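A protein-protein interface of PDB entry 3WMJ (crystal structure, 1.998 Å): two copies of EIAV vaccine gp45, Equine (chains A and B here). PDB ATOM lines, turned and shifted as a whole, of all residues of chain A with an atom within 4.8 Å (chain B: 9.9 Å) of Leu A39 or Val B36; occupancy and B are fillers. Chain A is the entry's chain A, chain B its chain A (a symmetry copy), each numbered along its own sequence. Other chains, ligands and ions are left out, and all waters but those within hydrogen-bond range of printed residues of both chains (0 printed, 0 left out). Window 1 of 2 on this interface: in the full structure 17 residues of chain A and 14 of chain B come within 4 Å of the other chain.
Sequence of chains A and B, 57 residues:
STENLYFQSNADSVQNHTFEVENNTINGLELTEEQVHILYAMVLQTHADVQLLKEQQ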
ATOM      1  N   GLN A  35       1.967  -0.456 -15.282  1.00  0.00           N
ATOM      2  CA  GLN A  35       3.274  -0.517 -15.940  1.00  0.00           C
ATOM      3  C   GLN A  35       4.376  -0.803 -14.930  1.00  0.00           C
ATOM      4  O   GLN A  35       5.335  -1.517 -15.224  1.00  0.00           O
ATOM      5  CB  GLN A  35       3.585   0.811 -16.610  1.00  0.00           C
ATOM      6  CG  GLN A  35       2.792   1.082 -17.869  1.00  0.00           C
ATOM      7  CD  GLN A  35       3.055   2.473 -18.324  1.00  0.00           C
ATOM      8  OE1 GLN A  35       2.983   3.401 -17.516  1.00  0.00           O
ATOM      9  NE2 GLN A  35       3.430   2.640 -19.584  1.00  0.00           N
ATOM     10  N   VAL A  36       4.233  -0.229 -13.739  1.00  0.00           N
ATOM     11  CA  VAL A  36       5.218  -0.407 -12.674  1.00  0.00           C
ATOM     12  C   VAL A  36       5.240  -1.875 -12.226  1.00  0.00           C
ATOM     13  O   VAL A  36       6.306  -2.433 -11.946  1.00  0.00           O
ATOM     14  CB  VAL A  36       4.928   0.560 -11.499  1.00  0.00           C
ATOM     15  CG1 VAL A  36       5.612   0.110 -10.215  1.00  0.00           C
ATOM     16  CG2 VAL A  36       5.359   2.001 -11.866  1.00  0.00           C
ATOM     17  N   HIS A  37       4.069  -2.507 -12.192  1.00  0.00           N
ATOM     18  CA  HIS A  37       3.982  -3.930 -11.853  1.00  0.00           C
ATOM     19  C   HIS A  37       4.711  -4.792 -12.885  1.00  0.00           C
ATOM     20  O   HIS A  37       5.368  -5.782 -12.541  1.00  0.00           O
ATOM     21  CB  HIS A  37       2.525  -4.388 -11.754  1.00  0.00           C
ATOM     22  CG  HIS A  37       1.814  -3.887 -10.542  1.00  0.00           C
ATOM     23  ND1 HIS A  37       0.436  -3.868 -10.448  1.00  0.00           N
ATOM     24  CD2 HIS A  37       2.275  -3.374  -9.379  1.00  0.00           C
ATOM     25  CE1 HIS A  37       0.083  -3.372  -9.275  1.00  0.00           C
ATOM     26  NE2 HIS A  37       1.180  -3.068  -8.603  1.00  0.00           N
ATOM     27  N   ILE A  38       4.579  -4.427 -14.154  1.00  0.00           N
ATOM     28  CA  ILE A  38       5.245  -5.156 -15.221  1.00  0.00           C
ATOM     29  C   ILE A  38       6.768  -4.982 -15.167  1.00  0.00           C
ATOM     30  O   ILE A  38       7.528  -5.958 -15.308  1.00  0.00           O
ATOM     31  CB  ILE A  38       4.718  -4.713 -16.599  1.00  0.00           C
ATOM     32  CG1 ILE A  38       3.274  -5.165 -16.782  1.00  0.00           C
ATOM     33  CG2 ILE A  38       5.569  -5.286 -17.707  1.00  0.00           C
ATOM     34  CD1 ILE A  38       2.536  -4.385 -17.870  1.00  0.00           C
ATOM     35  N   LEU A  39       7.208  -3.745 -14.965  1.00  0.00           N
ATOM     36  CA  LEU A  39       8.626  -3.431 -14.864  1.00  0.00           C
ATOM     37  C   LEU A  39       9.214  -4.208 -13.707  1.00  0.00           C
ATOM     38  O   LEU A  39      10.311  -4.769 -13.818  1.00  0.00           O
ATOM     39  CB  LEU A  39       8.821  -1.933 -14.607  1.00  0.00           C
ATOM     40  CG  LEU A  39       8.590  -1.030 -15.809  1.00  0.00           C
ATOM     41  CD1 LEU A  39       8.788   0.437 -15.434  1.00  0.00           C
ATOM     42  CD2 LEU A  39       9.572  -1.414 -16.930  1.00  0.00           C
ATOM     43  N   TYR A  40       8.474  -4.250 -12.601  1.00  0.00           N
ATOM     44  CA  TYR A  40       8.895  -4.958 -11.394  1.00  0.00           C
ATOM     45  C   TYR A  40       9.063  -6.439 -11.688  1.00  0.00           C
ATOM     46  O   TYR A  40      10.041  -7.054 -11.274  1.00  0.00           O
ATOM     47  CB  TYR A  40       7.851  -4.759 -10.294  1.00  0.00           C
ATOM     48  CG  TYR A  40       8.163  -5.425  -8.970  1.00  0.00           C
ATOM     49  CD1 TYR A  40       9.409  -5.291  -8.378  1.00  0.00           C
ATOM     50  CD2 TYR A  40       7.180  -6.138  -8.279  1.00  0.00           C
ATOM     51  CE1 TYR A  40       9.695  -5.888  -7.153  1.00  0.00           C
ATOM     52  CE2 TYR A  40       7.452  -6.734  -7.053  1.00  0.00           C
ATOM     53  CZ  TYR A  40       8.708  -6.599  -6.496  1.00  0.00           C
ATOM     54  OH  TYR A  40       8.983  -7.189  -5.283  1.00  0.00           O
ATOM     55  N   ALA A  41       8.105  -7.011 -12.404  1.00  0.00           N
ATOM     56  CA  ALA A  41       8.220  -8.408 -12.821  1.00  0.00           C
ATOM     57  C   ALA A  41       9.442  -8.645 -13.710  1.00  0.00           C
ATOM     58  O   ALA A  41      10.204  -9.599 -13.487  1.00  0.00           O
ATOM     59  CB  ALA A  41       6.967  -8.844 -13.533  1.00  0.00           C
ATOM     60  N   MET A  42       9.620  -7.795 -14.727  1.00  0.00           N
ATOM     61  CA  MET A  42      10.767  -7.919 -15.631  1.00  0.00           C
ATOM     62  C   MET A  42      12.092  -7.829 -14.869  1.00  0.00           C
ATOM     63  O   MET A  42      13.028  -8.589 -15.143  1.00  0.00           O
ATOM     64  CB  MET A  42      10.713  -6.854 -16.740  1.00  0.00           C
ATOM     65  CG  MET A  42       9.430  -6.915 -17.576  1.00  0.00           C
ATOM     66  SD  MET A  42       9.187  -5.496 -18.668  1.00  0.00           S
ATOM     67  CE  MET A  42       9.933  -6.101 -20.186  1.00  0.00           C
ATOM     68  N   VAL A  43      12.154  -6.901 -13.918  1.00  0.00           N
ATOM     69  CA  VAL A  43      13.343  -6.669 -13.108  1.00  0.00           C
ATOM     70  C   VAL A  43      13.656  -7.872 -12.212  1.00  0.00           C
ATOM     71  O   VAL A  43      14.818  -8.264 -12.071  1.00  0.00           O
ATOM     72  CB  VAL A  43      13.170  -5.398 -12.237  1.00  0.00           C
ATOM     73  CG1 VAL A  43      14.228  -5.339 -11.136  1.00  0.00           C
ATOM     74  CG2 VAL A  43      13.235  -4.148 -13.095  1.00  0.00           C
ATOM     75  N   GLY B  28       2.541  15.933 -13.423  1.00  0.00           N
ATOM     76  CA  GLY B  28       3.261  14.974 -12.603  1.00  0.00           C
ATOM     77  C   GLY B  28       3.133  13.564 -13.146  1.00  0.00           C
ATOM     78  O   GLY B  28       4.110  12.808 -13.146  1.00  0.00           O
ATOM     79  N   LEU B  29       1.926  13.204 -13.583  1.00  0.00           N
ATOM     80  CA  LEU B  29       1.670  11.902 -14.163  1.00  0.00           C
ATOM     81  C   LEU B  29       2.502  11.776 -15.411  1.00  0.00           C
ATOM     82  O   LEU B  29       3.101  10.741 -15.659  1.00  0.00           O
ATOM     83  CB  LEU B  29       0.200  11.767 -14.556  1.00  0.00           C
ATOM     84  CG  LEU B  29      -0.698  10.942 -13.658  1.00  0.00           C
ATOM     85  CD1 LEU B  29      -2.143  11.059 -14.152  1.00  0.00           C
ATOM     86  CD2 LEU B  29      -0.236   9.482 -13.641  1.00  0.00           C
ATOM     87  N   GLU B  30       2.536  12.843 -16.204  1.00  0.00           N
ATOM     88  CA  GLU B  30       3.289  12.821 -17.453  1.00  0.00           C
ATOM     89  C   GLU B  30       4.776  12.624 -17.181  1.00  0.00           C
ATOM     90  O   GLU B  30       5.467  11.948 -17.948  1.00  0.00           O
ATOM     91  CB  GLU B  30       3.045  14.105 -18.246  1.00  0.00           C
ATOM     92  CG  GLU B  30       3.730  14.125 -19.606  1.00  0.00           C
ATOM     93  CD  GLU B  30       3.172  15.206 -20.519  1.00  0.00           C
ATOM     94  OE1 GLU B  30       3.351  16.411 -20.205  1.00  0.00           O
ATOM     95  OE2 GLU B  30       2.552  14.844 -21.546  1.00  0.00           O
ATOM     96  N   LEU B  31       5.264  13.188 -16.081  1.00  0.00           N
ATOM     97  CA  LEU B  31       6.677  13.033 -15.726  1.00  0.00           C
ATOM     98  C   LEU B  31       7.007  11.615 -15.265  1.00  0.00           C
ATOM     99  O   LEU B  31       8.057  11.078 -15.632  1.00  0.00           O
ATOM    100  CB  LEU B  31       7.103  14.045 -14.665  1.00  0.00           C
ATOM    101  CG  LEU B  31       7.132  15.512 -15.089  1.00  0.00           C
ATOM    102  CD1 LEU B  31       7.324  16.368 -13.848  1.00  0.00           C
ATOM    103  CD2 LEU B  31       8.264  15.736 -16.058  1.00  0.00           C
ATOM    104  N   THR B  32       6.137  11.020 -14.446  1.00  0.00           N
ATOM    105  CA  THR B  32       6.354   9.643 -13.997  1.00  0.00           C
ATOM    106  C   THR B  32       6.326   8.722 -15.196  1.00  0.00           C
ATOM    107  O   THR B  32       7.078   7.758 -15.255  1.00  0.00           O
ATOM    108  CB  THR B  32       5.323   9.152 -12.977  1.00  0.00           C
ATOM    109  OG1 THR B  32       4.000   9.263 -13.533  1.00  0.00           O
ATOM    110  CG2 THR B  32       5.418   9.972 -11.685  1.00  0.00           C
ATOM    111  N   GLU B  33       5.465   9.029 -16.162  1.00  0.00           N
ATOM    112  CA  GLU B  33       5.396   8.212 -17.367  1.00  0.00           C
ATOM    113  C   GLU B  33       6.684   8.276 -18.165  1.00  0.00           C
ATOM    114  O   GLU B  33       7.123   7.270 -18.751  1.00  0.00           O
ATOM    115  CB  GLU B  33       4.201   8.600 -18.241  1.00  0.00           C
ATOM    116  CG  GLU B  33       4.080   7.759 -19.522  1.00  0.00           C
ATOM    117  CD  GLU B  33       3.755   6.291 -19.244  1.00  0.00           C
ATOM    118  OE1 GLU B  33       3.524   5.930 -18.067  1.00  0.00           O
ATOM    119  OE2 GLU B  33       3.730   5.484 -20.200  1.00  0.00           O
ATOM    120  N   GLU B  34       7.314   9.445 -18.177  1.00  0.00           N
ATOM    121  CA  GLU B  34       8.597   9.579 -18.852  1.00  0.00           C
ATOM    122  C   GLU B  34       9.682   8.769 -18.148  1.00  0.00           C
ATOM    123  O   GLU B  34      10.519   8.155 -18.801  1.00  0.00           O
ATOM    124  CB  GLU B  34       9.014  11.047 -18.951  1.00  0.00           C
ATOM    125  CG  GLU B  34       8.133  11.865 -19.877  1.00  0.00           C
ATOM    126  CD  GLU B  34       8.783  13.185 -20.249  1.00  0.00           C
ATOM    127  OE1 GLU B  34      10.029  13.293 -20.114  1.00  0.00           O
ATOM    128  OE2 GLU B  34       8.051  14.109 -20.677  1.00  0.00           O
ATOM    129  N   GLN B  35       9.666   8.755 -16.819  1.00  0.00           N
ATOM    130  CA  GLN B  35      10.621   7.930 -16.073  1.00  0.00           C
ATOM    131  C   GLN B  35      10.392   6.451 -16.353  1.00  0.00           C
ATOM    132  O   GLN B  35      11.339   5.669 -16.432  1.00  0.00           O
ATOM    133  CB  GLN B  35      10.455   8.157 -14.580  1.00  0.00           C
ATOM    134  CG  GLN B  35      10.979   9.485 -14.083  1.00  0.00           C
ATOM    135  CD  GLN B  35      10.601   9.659 -12.656  1.00  0.00           C
ATOM    136  OE1 GLN B  35       9.437   9.454 -12.306  1.00  0.00           O
ATOM    137  NE2 GLN B  35      11.569   9.962 -11.803  1.00  0.00           N
ATOM    138  N   VAL B  36       9.123   6.077 -16.490  1.00  0.00           N
ATOM    139  CA  VAL B  36       8.753   4.688 -16.751  1.00  0.00           C
ATOM    140  C   VAL B  36       9.274   4.261 -18.130  1.00  0.00           C
ATOM    141  O   VAL B  36       9.737   3.129 -18.307  1.00  0.00           O
ATOM    142  CB  VAL B  36       7.221   4.501 -16.620  1.00  0.00           C
ATOM    143  CG1 VAL B  36       6.746   3.231 -17.314  1.00  0.00           C
ATOM    144  CG2 VAL B  36       6.803   4.492 -15.129  1.00  0.00           C
ATOM    145  N   HIS B  37       9.232   5.177 -19.095  1.00  0.00           N
ATOM    146  CA  HIS B  37       9.773   4.903 -20.429  1.00  0.00           C
ATOM    147  C   HIS B  37      11.281   4.655 -20.376  1.00  0.00           C
ATOM    148  O   HIS B  37      11.812   3.789 -21.083  1.00  0.00           O
ATOM    149  CB  HIS B  37       9.487   6.059 -21.391  1.00  0.00           C
ATOM    150  CG  HIS B  37       8.058   6.157 -21.811  1.00  0.00           C
ATOM    151  ND1 HIS B  37       7.526   7.308 -22.358  1.00  0.00           N
ATOM    152  CD2 HIS B  37       7.043   5.265 -21.758  1.00  0.00           C
ATOM    153  CE1 HIS B  37       6.248   7.115 -22.629  1.00  0.00           C
ATOM    154  NE2 HIS B  37       5.929   5.880 -22.279  1.00  0.00           N
ATOM    155  N   ILE B  38      11.975   5.427 -19.550  1.00  0.00           N
ATOM    156  CA  ILE B  38      13.412   5.267 -19.396  1.00  0.00           C
ATOM    157  C   ILE B  38      13.769   3.945 -18.709  1.00  0.00           C
ATOM    158  O   ILE B  38      14.688   3.226 -19.144  1.00  0.00           O
ATOM    159  CB  ILE B  38      14.013   6.446 -18.607  1.00  0.00           C
ATOM    160  CG1 ILE B  38      13.939   7.726 -19.430  1.00  0.00           C
ATOM    161  CG2 ILE B  38      15.451   6.166 -18.240  1.00  0.00           C
ATOM    162  CD1 ILE B  38      14.059   8.992 -18.581  1.00  0.00           C
ATOM    163  N   LEU B  39      13.047   3.628 -17.641  1.00  0.00           N
ATOM    164  CA  LEU B  39      13.255   2.391 -16.900  1.00  0.00           C
ATOM    165  C   LEU B  39      13.032   1.223 -17.835  1.00  0.00           C
ATOM    166  O   LEU B  39      13.798   0.252 -17.823  1.00  0.00           O
ATOM    167  CB  LEU B  39      12.259   2.295 -15.739  1.00  0.00           C
ATOM    168  CG  LEU B  39      12.560   3.192 -14.546  1.00  0.00           C
ATOM    169  CD1 LEU B  39      11.496   3.032 -13.463  1.00  0.00           C
ATOM    170  CD2 LEU B  39      13.941   2.830 -13.974  1.00  0.00           C
ATOM    171  N   TYR B  40      11.988   1.328 -18.654  1.00  0.00           N
ATOM    172  CA  TYR B  40      11.633   0.289 -19.620  1.00  0.00           C
ATOM    173  C   TYR B  40      12.764   0.091 -20.614  1.00  0.00           C
ATOM    174  O   TYR B  40      13.131  -1.037 -20.930  1.00  0.00           O
ATOM    175  CB  TYR B  40      10.354   0.691 -20.355  1.00  0.00           C
ATOM    176  CG  TYR B  40       9.852  -0.304 -21.382  1.00  0.00           C
ATOM    177  CD1 TYR B  40       9.740  -1.651 -21.076  1.00  0.00           C
ATOM    178  CD2 TYR B  40       9.426   0.121 -22.642  1.00  0.00           C
ATOM    179  CE1 TYR B  40       9.264  -2.567 -22.011  1.00  0.00           C
ATOM    180  CE2 TYR B  40       8.944  -0.782 -23.582  1.00  0.00           C
ATOM    181  CZ  TYR B  40       8.861  -2.122 -23.256  1.00  0.00           C
ATOM    182  OH  TYR B  40       8.386  -3.020 -24.183  1.00  0.00           O
ATOM    183  N   ALA B  41      13.317   1.191 -21.107  1.00  0.00           N
ATOM    184  CA  ALA B  41      14.473   1.108 -21.996  1.00  0.00           C
ATOM    185  C   ALA B  41      15.674   0.446 -21.320  1.00  0.00           C
ATOM    186  O   ALA B  41      16.309  -0.447 -21.904  1.00  0.00           O
ATOM    187  CB  ALA B  41      14.847   2.479 -22.493  1.00  0.00           C
ATOM    188  N   MET B  42      16.002   0.892 -20.103  1.00  0.00           N
ATOM    189  CA  MET B  42      17.124   0.317 -19.357  1.00  0.00           C
ATOM    190  C   MET B  42      16.936  -1.186 -19.135  1.00  0.00           C
ATOM    191  O   MET B  42      17.887  -1.966 -19.269  1.00  0.00           O
ATOM    192  CB  MET B  42      17.319   1.037 -18.011  1.00  0.00           C
ATOM    193  CG  MET B  42      17.559   2.544 -18.160  1.00  0.00           C
ATOM    194  SD  MET B  42      17.475   3.465 -16.607  1.00  0.00           S
ATOM    195  CE  MET B  42      19.203   3.470 -16.119  1.00  0.00           C
ATOM    196  N   VAL B  43      15.710  -1.576 -18.800  1.00  0.00           N
ATOM    197  CA  VAL B  43      15.360  -2.966 -18.538  1.00  0.00           C
ATOM    198  C   VAL B  43      15.488  -3.826 -19.799  1.00  0.00           C
ATOM    199  O   VAL B  43      15.990  -4.953 -19.742  1.00  0.00           O
ATOM    200  CB  VAL B  43      13.917  -3.069 -17.979  1.00  0.00           C
ATOM    201  CG1 VAL B  43      13.407  -4.507 -18.038  1.00  0.00           C
ATOM    202  CG2 VAL B  43      13.856  -2.548 -16.554  1.00  0.00           C
ATOM    203  N   LEU B  44      15.023  -3.305 -20.933  1.00  0.00           N
ATOM    204  CA  LEU B  44      15.137  -4.024 -22.198  1.00  0.00           C
ATOM    205  C   LEU B  44      16.608  -4.203 -22.571  1.00  0.00           C
ATOM    206  O   LEU B  44      17.012  -5.260 -23.041  1.00  0.00           O
ATOM    207  CB  LEU B  44      14.401  -3.286 -23.321  1.00  0.00           C
ATOM    208  CG  LEU B  44      12.878  -3.334 -23.321  1.00  0.00           C
ATOM    209  CD1 LEU B  44      12.322  -2.487 -24.467  1.00  0.00           C
ATOM    210  CD2 LEU B  44      12.375  -4.765 -23.416  1.00  0.00           C
ATOM    211  N   GLN B  45      17.408  -3.168 -22.358  1.00  0.00           N
ATOM    212  CA  GLN B  45      18.821  -3.215 -22.724  1.00  0.00           C
ATOM    213  C   GLN B  45      19.570  -4.229 -21.868  1.00  0.00           C
ATOM    214  O   GLN B  45      20.403  -4.990 -22.377  1.00  0.00           O
ATOM    215  CB  GLN B  45      19.451  -1.829 -22.586  1.00  0.00           C
ATOM    216  CG  GLN B  45      20.977  -1.830 -22.705  1.00  0.00           C
ATOM    217  CD  GLN B  45      21.439  -2.092 -24.123  1.00  0.00           C
ATOM    218  OE1 GLN B  45      20.870  -1.555 -25.080  1.00  0.00           O
ATOM    219  NE2 GLN B  45      22.474  -2.921 -24.269  1.00  0.00           N
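Of the 18 printed residues of chain B, 5 touch a printed residue of chain A.
Printed residues of chain B that touch a printed residue of chain A: Glu B33, Val B36, Leu B39, Tyr B40 and Val B43.
Hydrophobic or aromatic side chains of chain B that line the printed part of chain A: Val B36, Leu B39 and Val B43.
Printed residues of chain A that touch a printed residue of chain B: Gln A35, Leu A39, Met A42 and Val A43.
Hydrophobic or aromatic side chains of chain A that line the printed part of chain B: Leu A39, Met A42 and Val A43.
The side-chain amide oxygen of Gln A35 sits close to the side-chain carboxylate of Glu B33.
Of the printed residues of chain B, Gln A35 touches Glu B33 and Val B36.
No residue of chain B comes within 4 Å of Val A36.
Ile A38 touches none of the printed residues of chain B.
Leu A39 touches just these residues of chain B: Val B36, Leu B39 and Tyr B40.
No residue of chain B comes within 4 Å of Ala A41.
Printed residues of chain B within 4 Å of Val A43: Val B43.
Gly B28 touches none of the printed residues of chain A.
Val B36 touches two residues of chain A.
Printed residues of chain A within 4 Å of Val B43: Met A42 and Val A43.
The nearest residue of chain B that does not touch Leu A39 is Val B43 (4.4 Å).
The nearest residue of chain A that does not touch Val B36 is Val A36 (4.4 Å).
The nearest printed residue of chain A that does not touch Glu B33 is Val A36 (7.6 Å).
Among the printed residues, pairs that only touch across the chains: Gln A35 with Val B36 (3.8 Å), Leu A39 with Val B36 (3.9 Å), Leu A39 with Leu B39 (3.9 Å), Leu A39 with Tyr B40 (3.8 Å), Met A42 with Val B43 (3.8 Å) and Val A43 with Val B43 (3.9 Å).
Gln A35 touches Val B36, but with the chains exchanged Val A36 does not touch Gln B35 (8.1 Å).
Leu A39 touches Val B36, but with the chains exchanged Val A36 does not touch Leu B39 (6.4 Å).
Met A42 touches Val B43, but with the chains exchanged Val A43 does not touch Met B42 (7.7 Å).
Val A43 touches its own counterpart, Val B43.
9 positions are printed for both chains.
Of the 7 pairs that touch across the chains among the printed residues, 2 have their exchanged pair printed and touching as well.
OE2 of Glu B33 is in hydrogen-bond range of NE2 of His B37 (3.1 Å).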
